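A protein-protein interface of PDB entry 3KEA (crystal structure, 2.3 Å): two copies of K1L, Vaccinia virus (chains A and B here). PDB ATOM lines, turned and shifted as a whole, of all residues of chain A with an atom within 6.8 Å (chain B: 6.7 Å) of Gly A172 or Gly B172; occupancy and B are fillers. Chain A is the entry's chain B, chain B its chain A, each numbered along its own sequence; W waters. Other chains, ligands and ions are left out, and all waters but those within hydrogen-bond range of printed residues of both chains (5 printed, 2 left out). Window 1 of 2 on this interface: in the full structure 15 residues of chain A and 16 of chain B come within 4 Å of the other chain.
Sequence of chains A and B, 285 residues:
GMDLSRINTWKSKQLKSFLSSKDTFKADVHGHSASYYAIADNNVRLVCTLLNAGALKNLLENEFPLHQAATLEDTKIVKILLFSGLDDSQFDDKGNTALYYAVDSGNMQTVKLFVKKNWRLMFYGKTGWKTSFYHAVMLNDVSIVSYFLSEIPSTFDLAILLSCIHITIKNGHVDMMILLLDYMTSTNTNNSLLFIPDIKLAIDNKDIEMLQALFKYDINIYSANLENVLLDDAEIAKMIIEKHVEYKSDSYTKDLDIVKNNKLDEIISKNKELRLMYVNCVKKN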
ATOM      1  N   ASN A 140     -30.250  -7.322  -3.166  1.00  0.00           N
ATOM      2  CA  ASN A 140     -28.965  -7.887  -3.506  1.00  0.00           C
ATOM      3  C   ASN A 140     -29.103  -9.259  -4.170  1.00  0.00           C
ATOM      4  O   ASN A 140     -28.319 -10.171  -3.923  1.00  0.00           O
ATOM      5  CB  ASN A 140     -28.011  -7.894  -2.301  1.00  0.00           C
ATOM      6  CG  ASN A 140     -26.558  -8.080  -2.716  1.00  0.00           C
ATOM      7  OD1 ASN A 140     -26.178  -7.785  -3.865  1.00  0.00           O
ATOM      8  ND2 ASN A 140     -25.742  -8.596  -1.798  1.00  0.00           N
ATOM      9  N   ILE A 167     -27.951   2.696  -3.631  1.00  0.00           N
ATOM     10  CA  ILE A 167     -28.339   1.699  -2.637  1.00  0.00           C
ATOM     11  C   ILE A 167     -27.277   0.600  -2.527  1.00  0.00           C
ATOM     12  O   ILE A 167     -26.963   0.151  -1.428  1.00  0.00           O
ATOM     13  CB  ILE A 167     -29.801   1.150  -2.862  1.00  0.00           C
ATOM     14  CG1 ILE A 167     -30.378   0.566  -1.570  1.00  0.00           C
ATOM     15  CG2 ILE A 167     -29.850   0.097  -3.934  1.00  0.00           C
ATOM     16  CD1 ILE A 167     -30.939   1.614  -0.576  1.00  0.00           C
ATOM     17  N   THR A 168     -26.713   0.216  -3.669  1.00  0.00           N
ATOM     18  CA  THR A 168     -25.591  -0.705  -3.732  1.00  0.00           C
ATOM     19  C   THR A 168     -24.350  -0.233  -2.934  1.00  0.00           C
ATOM     20  O   THR A 168     -23.852  -0.987  -2.096  1.00  0.00           O
ATOM     21  CB  THR A 168     -25.207  -1.011  -5.192  1.00  0.00           C
ATOM     22  OG1 THR A 168     -26.302  -1.632  -5.875  1.00  0.00           O
ATOM     23  CG2 THR A 168     -24.049  -1.927  -5.244  1.00  0.00           C
ATOM     24  N   ILE A 169     -23.846   0.981  -3.185  1.00  0.00           N
ATOM     25  CA  ILE A 169     -22.662   1.481  -2.454  1.00  0.00           C
ATOM     26  C   ILE A 169     -23.000   1.627  -0.973  1.00  0.00           C
ATOM     27  O   ILE A 169     -22.256   1.174  -0.118  1.00  0.00           O
ATOM     28  CB  ILE A 169     -22.154   2.876  -2.938  1.00  0.00           C
ATOM     29  CG1 ILE A 169     -21.843   2.903  -4.443  1.00  0.00           C
ATOM     30  CG2 ILE A 169     -20.986   3.389  -2.064  1.00  0.00           C
ATOM     31  CD1 ILE A 169     -20.417   3.084  -4.841  1.00  0.00           C
ATOM     32  N   LYS A 170     -24.131   2.271  -0.688  1.00  0.00           N
ATOM     33  CA  LYS A 170     -24.608   2.463   0.668  1.00  0.00           C
ATOM     34  C   LYS A 170     -24.587   1.199   1.526  1.00  0.00           C
ATOM     35  O   LYS A 170     -24.200   1.274   2.679  1.00  0.00           O
ATOM     36  CB  LYS A 170     -26.012   3.047   0.646  1.00  0.00           C
ATOM     37  CG  LYS A 170     -26.419   3.754   1.920  1.00  0.00           C
ATOM     38  CD  LYS A 170     -27.942   3.886   1.947  1.00  0.00           C
ATOM     39  CE  LYS A 170     -28.482   4.167   3.349  1.00  0.00           C
ATOM     40  NZ  LYS A 170     -28.831   5.603   3.494  1.00  0.00           N
ATOM     41  N   ASN A 171     -24.994   0.057   0.966  1.00  0.00           N
ATOM     42  CA  ASN A 171     -25.171  -1.175   1.710  1.00  0.00           C
ATOM     43  C   ASN A 171     -24.095  -2.246   1.417  1.00  0.00           C
ATOM     44  O   ASN A 171     -24.212  -3.401   1.836  1.00  0.00           O
ATOM     45  CB  ASN A 171     -26.590  -1.746   1.481  1.00  0.00           C
ATOM     46  CG  ASN A 171     -27.711  -0.822   1.992  1.00  0.00           C
ATOM     47  OD1 ASN A 171     -27.737  -0.460   3.154  1.00  0.00           O
ATOM     48  ND2 ASN A 171     -28.652  -0.477   1.132  1.00  0.00           N
ATOM     49  N   GLY A 172     -23.051  -1.861   0.707  1.00  0.00           N
ATOM     50  CA  GLY A 172     -21.848  -2.683   0.629  1.00  0.00           C
ATOM     51  C   GLY A 172     -21.931  -3.885  -0.286  1.00  0.00           C
ATOM     52  O   GLY A 172     -21.286  -4.888  -0.034  1.00  0.00           O
ATOM     53  N   HIS A 173     -22.718  -3.793  -1.356  1.00  0.00           N
ATOM     54  CA  HIS A 173     -22.959  -4.936  -2.218  1.00  0.00           C
ATOM     55  C   HIS A 173     -21.987  -4.950  -3.394  1.00  0.00           C
ATOM     56  O   HIS A 173     -22.330  -4.490  -4.493  1.00  0.00           O
ATOM     57  CB  HIS A 173     -24.425  -4.920  -2.674  1.00  0.00           C
ATOM     58  CG  HIS A 173     -25.411  -4.972  -1.545  1.00  0.00           C
ATOM     59  ND1 HIS A 173     -26.606  -4.288  -1.569  1.00  0.00           N
ATOM     60  CD2 HIS A 173     -25.377  -5.620  -0.352  1.00  0.00           C
ATOM     61  CE1 HIS A 173     -27.271  -4.517  -0.450  1.00  0.00           C
ATOM     62  NE2 HIS A 173     -26.543  -5.314   0.310  1.00  0.00           N
ATOM     63  N   VAL A 174     -20.814  -5.496  -3.190  1.00  0.00           N
ATOM     64  CA  VAL A 174     -19.791  -5.348  -4.177  1.00  0.00           C
ATOM     65  C   VAL A 174     -19.944  -6.130  -5.471  1.00  0.00           C
ATOM     66  O   VAL A 174     -19.616  -5.636  -6.515  1.00  0.00           O
ATOM     67  CB  VAL A 174     -18.364  -5.255  -3.610  1.00  0.00           C
ATOM     68  CG1 VAL A 174     -18.375  -4.780  -2.204  1.00  0.00           C
ATOM     69  CG2 VAL A 174     -17.678  -6.497  -3.708  1.00  0.00           C
ATOM     70  N   ASP A 175     -20.486  -7.332  -5.389  1.00  0.00           N
ATOM     71  CA  ASP A 175     -20.756  -8.106  -6.601  1.00  0.00           C
ATOM     72  C   ASP A 175     -21.829  -7.431  -7.463  1.00  0.00           C
ATOM     73  O   ASP A 175     -21.752  -7.464  -8.690  1.00  0.00           O
ATOM     74  CB  ASP A 175     -21.135  -9.574  -6.311  1.00  0.00           C
ATOM     75  CG  ASP A 175     -19.938 -10.403  -5.858  1.00  0.00           C
ATOM     76  OD1 ASP A 175     -18.790 -10.096  -6.269  1.00  0.00           O
ATOM     77  OD2 ASP A 175     -20.132 -11.345  -5.053  1.00  0.00           O
ATOM     78  N   ASN A 205     -17.058   5.137   4.446  1.00  0.00           N
ATOM     79  CA  ASN A 205     -17.196   3.824   5.084  1.00  0.00           C
ATOM     80  C   ASN A 205     -15.880   3.087   5.066  1.00  0.00           C
ATOM     81  O   ASN A 205     -15.676   2.148   5.819  1.00  0.00           O
ATOM     82  CB  ASN A 205     -18.218   2.944   4.356  1.00  0.00           C
ATOM     83  CG  ASN A 205     -19.592   3.562   4.267  1.00  0.00           C
ATOM     84  OD1 ASN A 205     -20.018   4.331   5.145  1.00  0.00           O
ATOM     85  ND2 ASN A 205     -20.317   3.211   3.198  1.00  0.00           N
ATOM     86  N   ASP A 207     -14.668   0.848   2.854  1.00  0.00           N
ATOM     87  CA  ASP A 207     -14.843  -0.551   2.515  1.00  0.00           C
ATOM     88  C   ASP A 207     -13.782  -0.822   1.478  1.00  0.00           C
ATOM     89  O   ASP A 207     -13.920  -0.424   0.317  1.00  0.00           O
ATOM     90  CB  ASP A 207     -16.255  -0.752   1.953  1.00  0.00           C
ATOM     91  CG  ASP A 207     -16.562  -2.197   1.565  1.00  0.00           C
ATOM     92  OD1 ASP A 207     -17.740  -2.593   1.683  1.00  0.00           O
ATOM     93  OD2 ASP A 207     -15.667  -2.925   1.090  1.00  0.00           O
ATOM     94  N   GLU A 209     -12.661  -3.606  -0.090  1.00  0.00           N
ATOM     95  CA  GLU A 209     -13.039  -4.413  -1.258  1.00  0.00           C
ATOM     96  C   GLU A 209     -13.917  -3.627  -2.250  1.00  0.00           C
ATOM     97  O   GLU A 209     -13.736  -3.748  -3.473  1.00  0.00           O
ATOM     98  CB  GLU A 209     -13.696  -5.753  -0.880  1.00  0.00           C
ATOM     99  CG  GLU A 209     -13.615  -6.787  -2.026  1.00  0.00           C
ATOM    100  CD  GLU A 209     -14.549  -7.975  -1.880  1.00  0.00           C
ATOM    101  OE1 GLU A 209     -14.341  -9.000  -2.583  1.00  0.00           O
ATOM    102  OE2 GLU A 209     -15.495  -7.918  -1.073  1.00  0.00           O
ATOM    103  N   MET A 210     -14.841  -2.817  -1.718  1.00  0.00           N
ATOM    104  CA  MET A 210     -15.701  -1.946  -2.535  1.00  0.00           C
ATOM    105  C   MET A 210     -14.862  -0.949  -3.316  1.00  0.00           C
ATOM    106  O   MET A 210     -14.971  -0.877  -4.552  1.00  0.00           O
ATOM    107  CB  MET A 210     -16.748  -1.211  -1.678  1.00  0.00           C
ATOM    108  CG  MET A 210     -17.676  -0.237  -2.436  1.00  0.00           C
ATOM    109  SD  MET A 210     -18.934  -1.115  -3.670  1.00  0.00           S
ATOM    110  CE  MET A 210     -20.300  -1.619  -2.368  1.00  0.00           C
ATOM    111  N   ASN B 140     -13.182  -4.443   5.751  1.00  0.00           N
ATOM    112  CA  ASN B 140     -13.443  -5.347   4.636  1.00  0.00           C
ATOM    113  C   ASN B 140     -12.224  -5.473   3.739  1.00  0.00           C
ATOM    114  O   ASN B 140     -12.349  -5.424   2.530  1.00  0.00           O
ATOM    115  CB  ASN B 140     -14.687  -4.950   3.825  1.00  0.00           C
ATOM    116  CG  ASN B 140     -15.189  -6.074   2.894  1.00  0.00           C
ATOM    117  OD1 ASN B 140     -14.909  -7.263   3.104  1.00  0.00           O
ATOM    118  ND2 ASN B 140     -15.951  -5.694   1.863  1.00  0.00           N
ATOM    119  N   ILE B 167     -19.870  -8.027  12.660  1.00  0.00           N
ATOM    120  CA  ILE B 167     -19.593  -6.835  11.883  1.00  0.00           C
ATOM    121  C   ILE B 167     -19.731  -7.120  10.374  1.00  0.00           C
ATOM    122  O   ILE B 167     -20.354  -6.344   9.645  1.00  0.00           O
ATOM    123  CB  ILE B 167     -18.208  -6.266  12.302  1.00  0.00           C
ATOM    124  CG1 ILE B 167     -18.358  -4.930  13.071  1.00  0.00           C
ATOM    125  CG2 ILE B 167     -17.265  -6.146  11.153  1.00  0.00           C
ATOM    126  CD1 ILE B 167     -19.087  -3.761  12.348  1.00  0.00           C
ATOM    127  N   THR B 168     -19.168  -8.251   9.929  1.00  0.00           N
ATOM    128  CA  THR B 168     -19.326  -8.752   8.574  1.00  0.00           C
ATOM    129  C   THR B 168     -20.781  -8.890   8.116  1.00  0.00           C
ATOM    130  O   THR B 168     -21.166  -8.397   7.045  1.00  0.00           O
ATOM    131  CB  THR B 168     -18.625 -10.149   8.405  1.00  0.00           C
ATOM    132  OG1 THR B 168     -17.207 -10.023   8.616  1.00  0.00           O
ATOM    133  CG2 THR B 168     -18.842 -10.679   7.005  1.00  0.00           C
ATOM    134  N   ILE B 169     -21.608  -9.593   8.891  1.00  0.00           N
ATOM    135  CA  ILE B 169     -23.012  -9.700   8.513  1.00  0.00           C
ATOM    136  C   ILE B 169     -23.726  -8.345   8.651  1.00  0.00           C
ATOM    137  O   ILE B 169     -24.472  -7.978   7.736  1.00  0.00           O
ATOM    138  CB  ILE B 169     -23.744 -10.821   9.261  1.00  0.00           C
ATOM    139  CG1 ILE B 169     -23.184 -12.184   8.840  1.00  0.00           C
ATOM    140  CG2 ILE B 169     -25.224 -10.780   8.949  1.00  0.00           C
ATOM    141  CD1 ILE B 169     -23.792 -13.337   9.609  1.00  0.00           C
ATOM    142  N   LYS B 170     -23.510  -7.602   9.732  1.00  0.00           N
ATOM    143  CA  LYS B 170     -24.157  -6.292   9.893  1.00  0.00           C
ATOM    144  C   LYS B 170     -23.982  -5.400   8.665  1.00  0.00           C
ATOM    145  O   LYS B 170     -24.912  -4.716   8.282  1.00  0.00           O
ATOM    146  CB  LYS B 170     -23.627  -5.541  11.116  1.00  0.00           C
ATOM    147  CG  LYS B 170     -24.654  -4.634  11.755  1.00  0.00           C
ATOM    148  CD  LYS B 170     -24.186  -3.187  11.855  1.00  0.00           C
ATOM    149  CE  LYS B 170     -23.553  -2.847  13.200  1.00  0.00           C
ATOM    150  NZ  LYS B 170     -24.546  -2.909  14.285  1.00  0.00           N
ATOM    151  N   ASN B 171     -22.794  -5.418   8.061  1.00  0.00           N
ATOM    152  CA  ASN B 171     -22.423  -4.482   6.997  1.00  0.00           C
ATOM    153  C   ASN B 171     -22.342  -5.080   5.585  1.00  0.00           C
ATOM    154  O   ASN B 171     -21.856  -4.437   4.668  1.00  0.00           O
ATOM    155  CB  ASN B 171     -21.077  -3.822   7.299  1.00  0.00           C
ATOM    156  CG  ASN B 171     -21.081  -3.028   8.565  1.00  0.00           C
ATOM    157  OD1 ASN B 171     -21.831  -2.066   8.719  1.00  0.00           O
ATOM    158  ND2 ASN B 171     -20.212  -3.399   9.479  1.00  0.00           N
ATOM    159  N   GLY B 172     -22.810  -6.308   5.418  1.00  0.00           N
ATOM    160  CA  GLY B 172     -23.040  -6.873   4.096  1.00  0.00           C
ATOM    161  C   GLY B 172     -21.805  -7.358   3.332  1.00  0.00           C
ATOM    162  O   GLY B 172     -21.812  -7.339   2.083  1.00  0.00           O
ATOM    163  N   HIS B 173     -20.756  -7.805   4.047  1.00  0.00           N
ATOM    164  CA  HIS B 173     -19.487  -8.147   3.399  1.00  0.00           C
ATOM    165  C   HIS B 173     -19.408  -9.642   3.034  1.00  0.00           C
ATOM    166  O   HIS B 173     -18.795 -10.447   3.741  1.00  0.00           O
ATOM    167  CB  HIS B 173     -18.275  -7.689   4.227  1.00  0.00           C
ATOM    168  CG  HIS B 173     -18.282  -6.223   4.565  1.00  0.00           C
ATOM    169  ND1 HIS B 173     -17.899  -5.739   5.800  1.00  0.00           N
ATOM    170  CD2 HIS B 173     -18.639  -5.142   3.831  1.00  0.00           C
ATOM    171  CE1 HIS B 173     -18.005  -4.423   5.809  1.00  0.00           C
ATOM    172  NE2 HIS B 173     -18.457  -4.035   4.627  1.00  0.00           N
ATOM    173  N   VAL B 174     -20.041  -9.989   1.923  1.00  0.00           N
ATOM    174  CA  VAL B 174     -20.237 -11.378   1.550  1.00  0.00           C
ATOM    175  C   VAL B 174     -18.949 -12.167   1.385  1.00  0.00           C
ATOM    176  O   VAL B 174     -18.853 -13.263   1.943  1.00  0.00           O
ATOM    177  CB  VAL B 174     -21.190 -11.529   0.328  1.00  0.00           C
ATOM    178  CG1 VAL B 174     -21.413 -13.006  -0.032  1.00  0.00           C
ATOM    179  CG2 VAL B 174     -22.534 -10.847   0.647  1.00  0.00           C
ATOM    180  N   ASP B 175     -17.969 -11.629   0.647  1.00  0.00           N
ATOM    181  CA  ASP B 175     -16.687 -12.345   0.448  1.00  0.00           C
ATOM    182  C   ASP B 175     -15.904 -12.559   1.760  1.00  0.00           C
ATOM    183  O   ASP B 175     -15.235 -13.570   1.930  1.00  0.00           O
ATOM    184  CB  ASP B 175     -15.763 -11.657  -0.586  1.00  0.00           C
ATOM    185  CG  ASP B 175     -16.287 -11.755  -2.022  1.00  0.00           C
ATOM    186  OD1 ASP B 175     -16.980 -12.743  -2.353  1.00  0.00           O
ATOM    187  OD2 ASP B 175     -16.008 -10.829  -2.835  1.00  0.00           O
ATOM    188  N   ASN B 205     -32.463  -7.931   7.111  1.00  0.00           N
ATOM    189  CA  ASN B 205     -31.956  -7.112   6.011  1.00  0.00           C
ATOM    190  C   ASN B 205     -32.361  -7.700   4.663  1.00  0.00           C
ATOM    191  O   ASN B 205     -32.389  -7.005   3.658  1.00  0.00           O
ATOM    192  CB  ASN B 205     -30.420  -7.013   6.091  1.00  0.00           C
ATOM    193  CG  ASN B 205     -29.929  -6.301   7.363  1.00  0.00           C
ATOM    194  OD1 ASN B 205     -30.613  -5.428   7.922  1.00  0.00           O
ATOM    195  ND2 ASN B 205     -28.719  -6.663   7.809  1.00  0.00           N
ATOM    196  N   ASP B 207     -30.655  -9.728   2.602  1.00  0.00           N
ATOM    197  CA  ASP B 207     -29.581  -9.630   1.633  1.00  0.00           C
ATOM    198  C   ASP B 207     -29.505 -10.989   0.949  1.00  0.00           C
ATOM    199  O   ASP B 207     -28.963 -11.931   1.521  1.00  0.00           O
ATOM    200  CB  ASP B 207     -28.271  -9.282   2.343  1.00  0.00           C
ATOM    201  CG  ASP B 207     -27.065  -9.202   1.388  1.00  0.00           C
ATOM    202  OD1 ASP B 207     -26.985  -9.956   0.393  1.00  0.00           O
ATOM    203  OD2 ASP B 207     -26.160  -8.405   1.662  1.00  0.00           O
ATOM    204  N   GLU B 209     -27.829 -12.314  -1.649  1.00  0.00           N
ATOM    205  CA  GLU B 209     -26.480 -12.881  -1.829  1.00  0.00           C
ATOM    206  C   GLU B 209     -25.853 -13.359  -0.503  1.00  0.00           C
ATOM    207  O   GLU B 209     -25.215 -14.403  -0.456  1.00  0.00           O
ATOM    208  CB  GLU B 209     -25.528 -11.912  -2.571  1.00  0.00           C
ATOM    209  CG  GLU B 209     -24.395 -12.658  -3.287  1.00  0.00           C
ATOM    210  CD  GLU B 209     -23.249 -11.792  -3.746  1.00  0.00           C
ATOM    211  OE1 GLU B 209     -22.447 -12.299  -4.569  1.00  0.00           O
ATOM    212  OE2 GLU B 209     -23.120 -10.622  -3.306  1.00  0.00           O
ATOM    213  N   MET B 210     -26.023 -12.579   0.565  1.00  0.00           N
ATOM    214  CA  MET B 210     -25.494 -12.946   1.872  1.00  0.00           C
ATOM    215  C   MET B 210     -26.155 -14.234   2.373  1.00  0.00           C
ATOM    216  O   MET B 210     -25.446 -15.173   2.770  1.00  0.00           O
ATOM    217  CB  MET B 210     -25.659 -11.800   2.877  1.00  0.00           C
ATOM    218  CG  MET B 210     -25.271 -12.093   4.346  1.00  0.00           C
ATOM    219  SD  MET B 210     -23.336 -12.238   4.506  1.00  0.00           S
ATOM    220  CE  MET B 210     -22.919 -10.327   4.365  1.00  0.00           C
HETATM  221  O   HOH W   1     -20.441  -9.402  -3.191  1.00  0.00           O
HETATM  222  O   HOH W   2     -16.396  -8.829   1.766  1.00  0.00           O
HETATM  223  O   HOH W   3     -23.604  -7.756  -4.097  1.00  0.00           O
HETATM  224  O   HOH W   4     -20.379  -7.653  -0.603  1.00  0.00           O
HETATM  225  O   HOH W   5     -16.479 -12.527  -5.687  1.00  0.00           O
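Asn A140 touches Glu B209, and with the chains exchanged Glu A209 touches Asn B140.
Gly B172 touches its own counterpart, Gly A172.
His A173 touches Asp B207, and with the chains exchanged Asp A207 touches His B173.
Asp A175 touches Glu B209, and with the chains exchanged Glu A209 touches Asp B175.
O of Asn A171 touches O of Asn B171, at 3.8 Å.
O of Asn B140 is in hydrogen-bond range of N of Glu A209.
The backbone carbonyl oxygen of Gly A172 sits close to the backbone carbonyl oxygen of Gly B172, at 3.3 Å.
The side-chain carboxylate of Asp A207 sits at hydrogen-bond distance from the side-chain amide nitrogen of Asn B140 (2.9 Å).
The backbone NH of Glu B209 lies within hydrogen-bond range of the backbone carbonyl oxygen of Asn A140 (3.2 Å).
OD1 of Asp B207 sits at hydrogen-bond distance from ND2 of Asn A140 (2.9 Å).
OD2 of Asp A175 sits close to OE1 of Glu B209.
OD1 of Asp A207 lies within hydrogen-bond range of NE2 of His B173 (3.4 Å).
The side-chain carboxylate (OD2) of Asp B175 lies close to the side-chain carboxylate (OE1) of Glu A209.
The side-chain carboxylate (OD2) of Asp B207 is in hydrogen-bond range of a ring nitrogen (NE2) of His A173.
Hydrophobic or aromatic side chains of chain B within 4 Å of the printed part of chain A: His B173.
Of the 14 printed residues of chain A, 7 touch a printed residue of chain B.
Printed residues of chain A that touch a printed residue of chain B: Asn A140, Asn A171, Gly A172, His A173, Asp A175, Asp A207 and Glu A209.
Hydrophobic or aromatic side chains of chain A within 4 Å of the printed part of chain B: His A173.
Thr A168 touches none of the printed residues of chain B.
Of the printed residues of chain B, Asn A171 touches Asn B171 (3.8 Å).
Of chain B, only Gly B172 comes within 4 Å of Gly A172.
Of the printed residues of chain B, His A173 touches Asp B207 (3.4 Å).
Met A210 touches none of the printed residues of chain B.
Of chain A, only Gly A172 (3.3 Å) comes within 4 Å of Gly B172.
Of the printed residues of chain A, His B173 touches Asp A207 (3.4 Å).
Printed residues of chain A within 4 Å of Asp B175: Glu A209.
The nearest residue of chain A that does not touch Gly B172 is Asn A171 (4.3 Å).
Water W2 lies within hydrogen-bond range of OD1 of Asn B140 (2.5 Å), OE2 of Glu A209 (3.1 Å) and N of Asp B175 (3.4 Å).
Water W3 lies within hydrogen-bond range of OD1 of Asn A140, OE2 of Glu B209 and N of Asp A175.
Water W1 bridges OD2 of Asp A175 and OE2 of Glu B209.
Water W4 lies within hydrogen-bond range of O of Gly A172 (3.0 Å), O of Gly B172 (3.1 Å), N of Val A174 (3.4 Å) and N of Val B174 (3.5 Å).
Water W5 bridges the side-chain carboxylate (OD2) of Asp B175 (3.4 Å) and the side-chain carboxylate (OD1) of Asp A175 (3.4 Å).
The side-chain carboxylate (OD2) of Asp A207 sits at hydrogen-bond distance from the backbone NH (N) of Glu A209.
N of His A173 sits at hydrogen-bond distance from O of Thr A168.
N of Glu B209 is in hydrogen-bond range of OD1 of Asp B207 (3.2 Å).
O of Ile A167 sits at hydrogen-bond distance from ND2 of Asn A171 (3.1 Å).
The backbone NH of His B173 is in hydrogen-bond range of the backbone carbonyl oxygen of Thr B168 (3.1 Å).
O of Ile B167 lies within hydrogen-bond range of ND2 of Asn B171 (3.0 Å).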
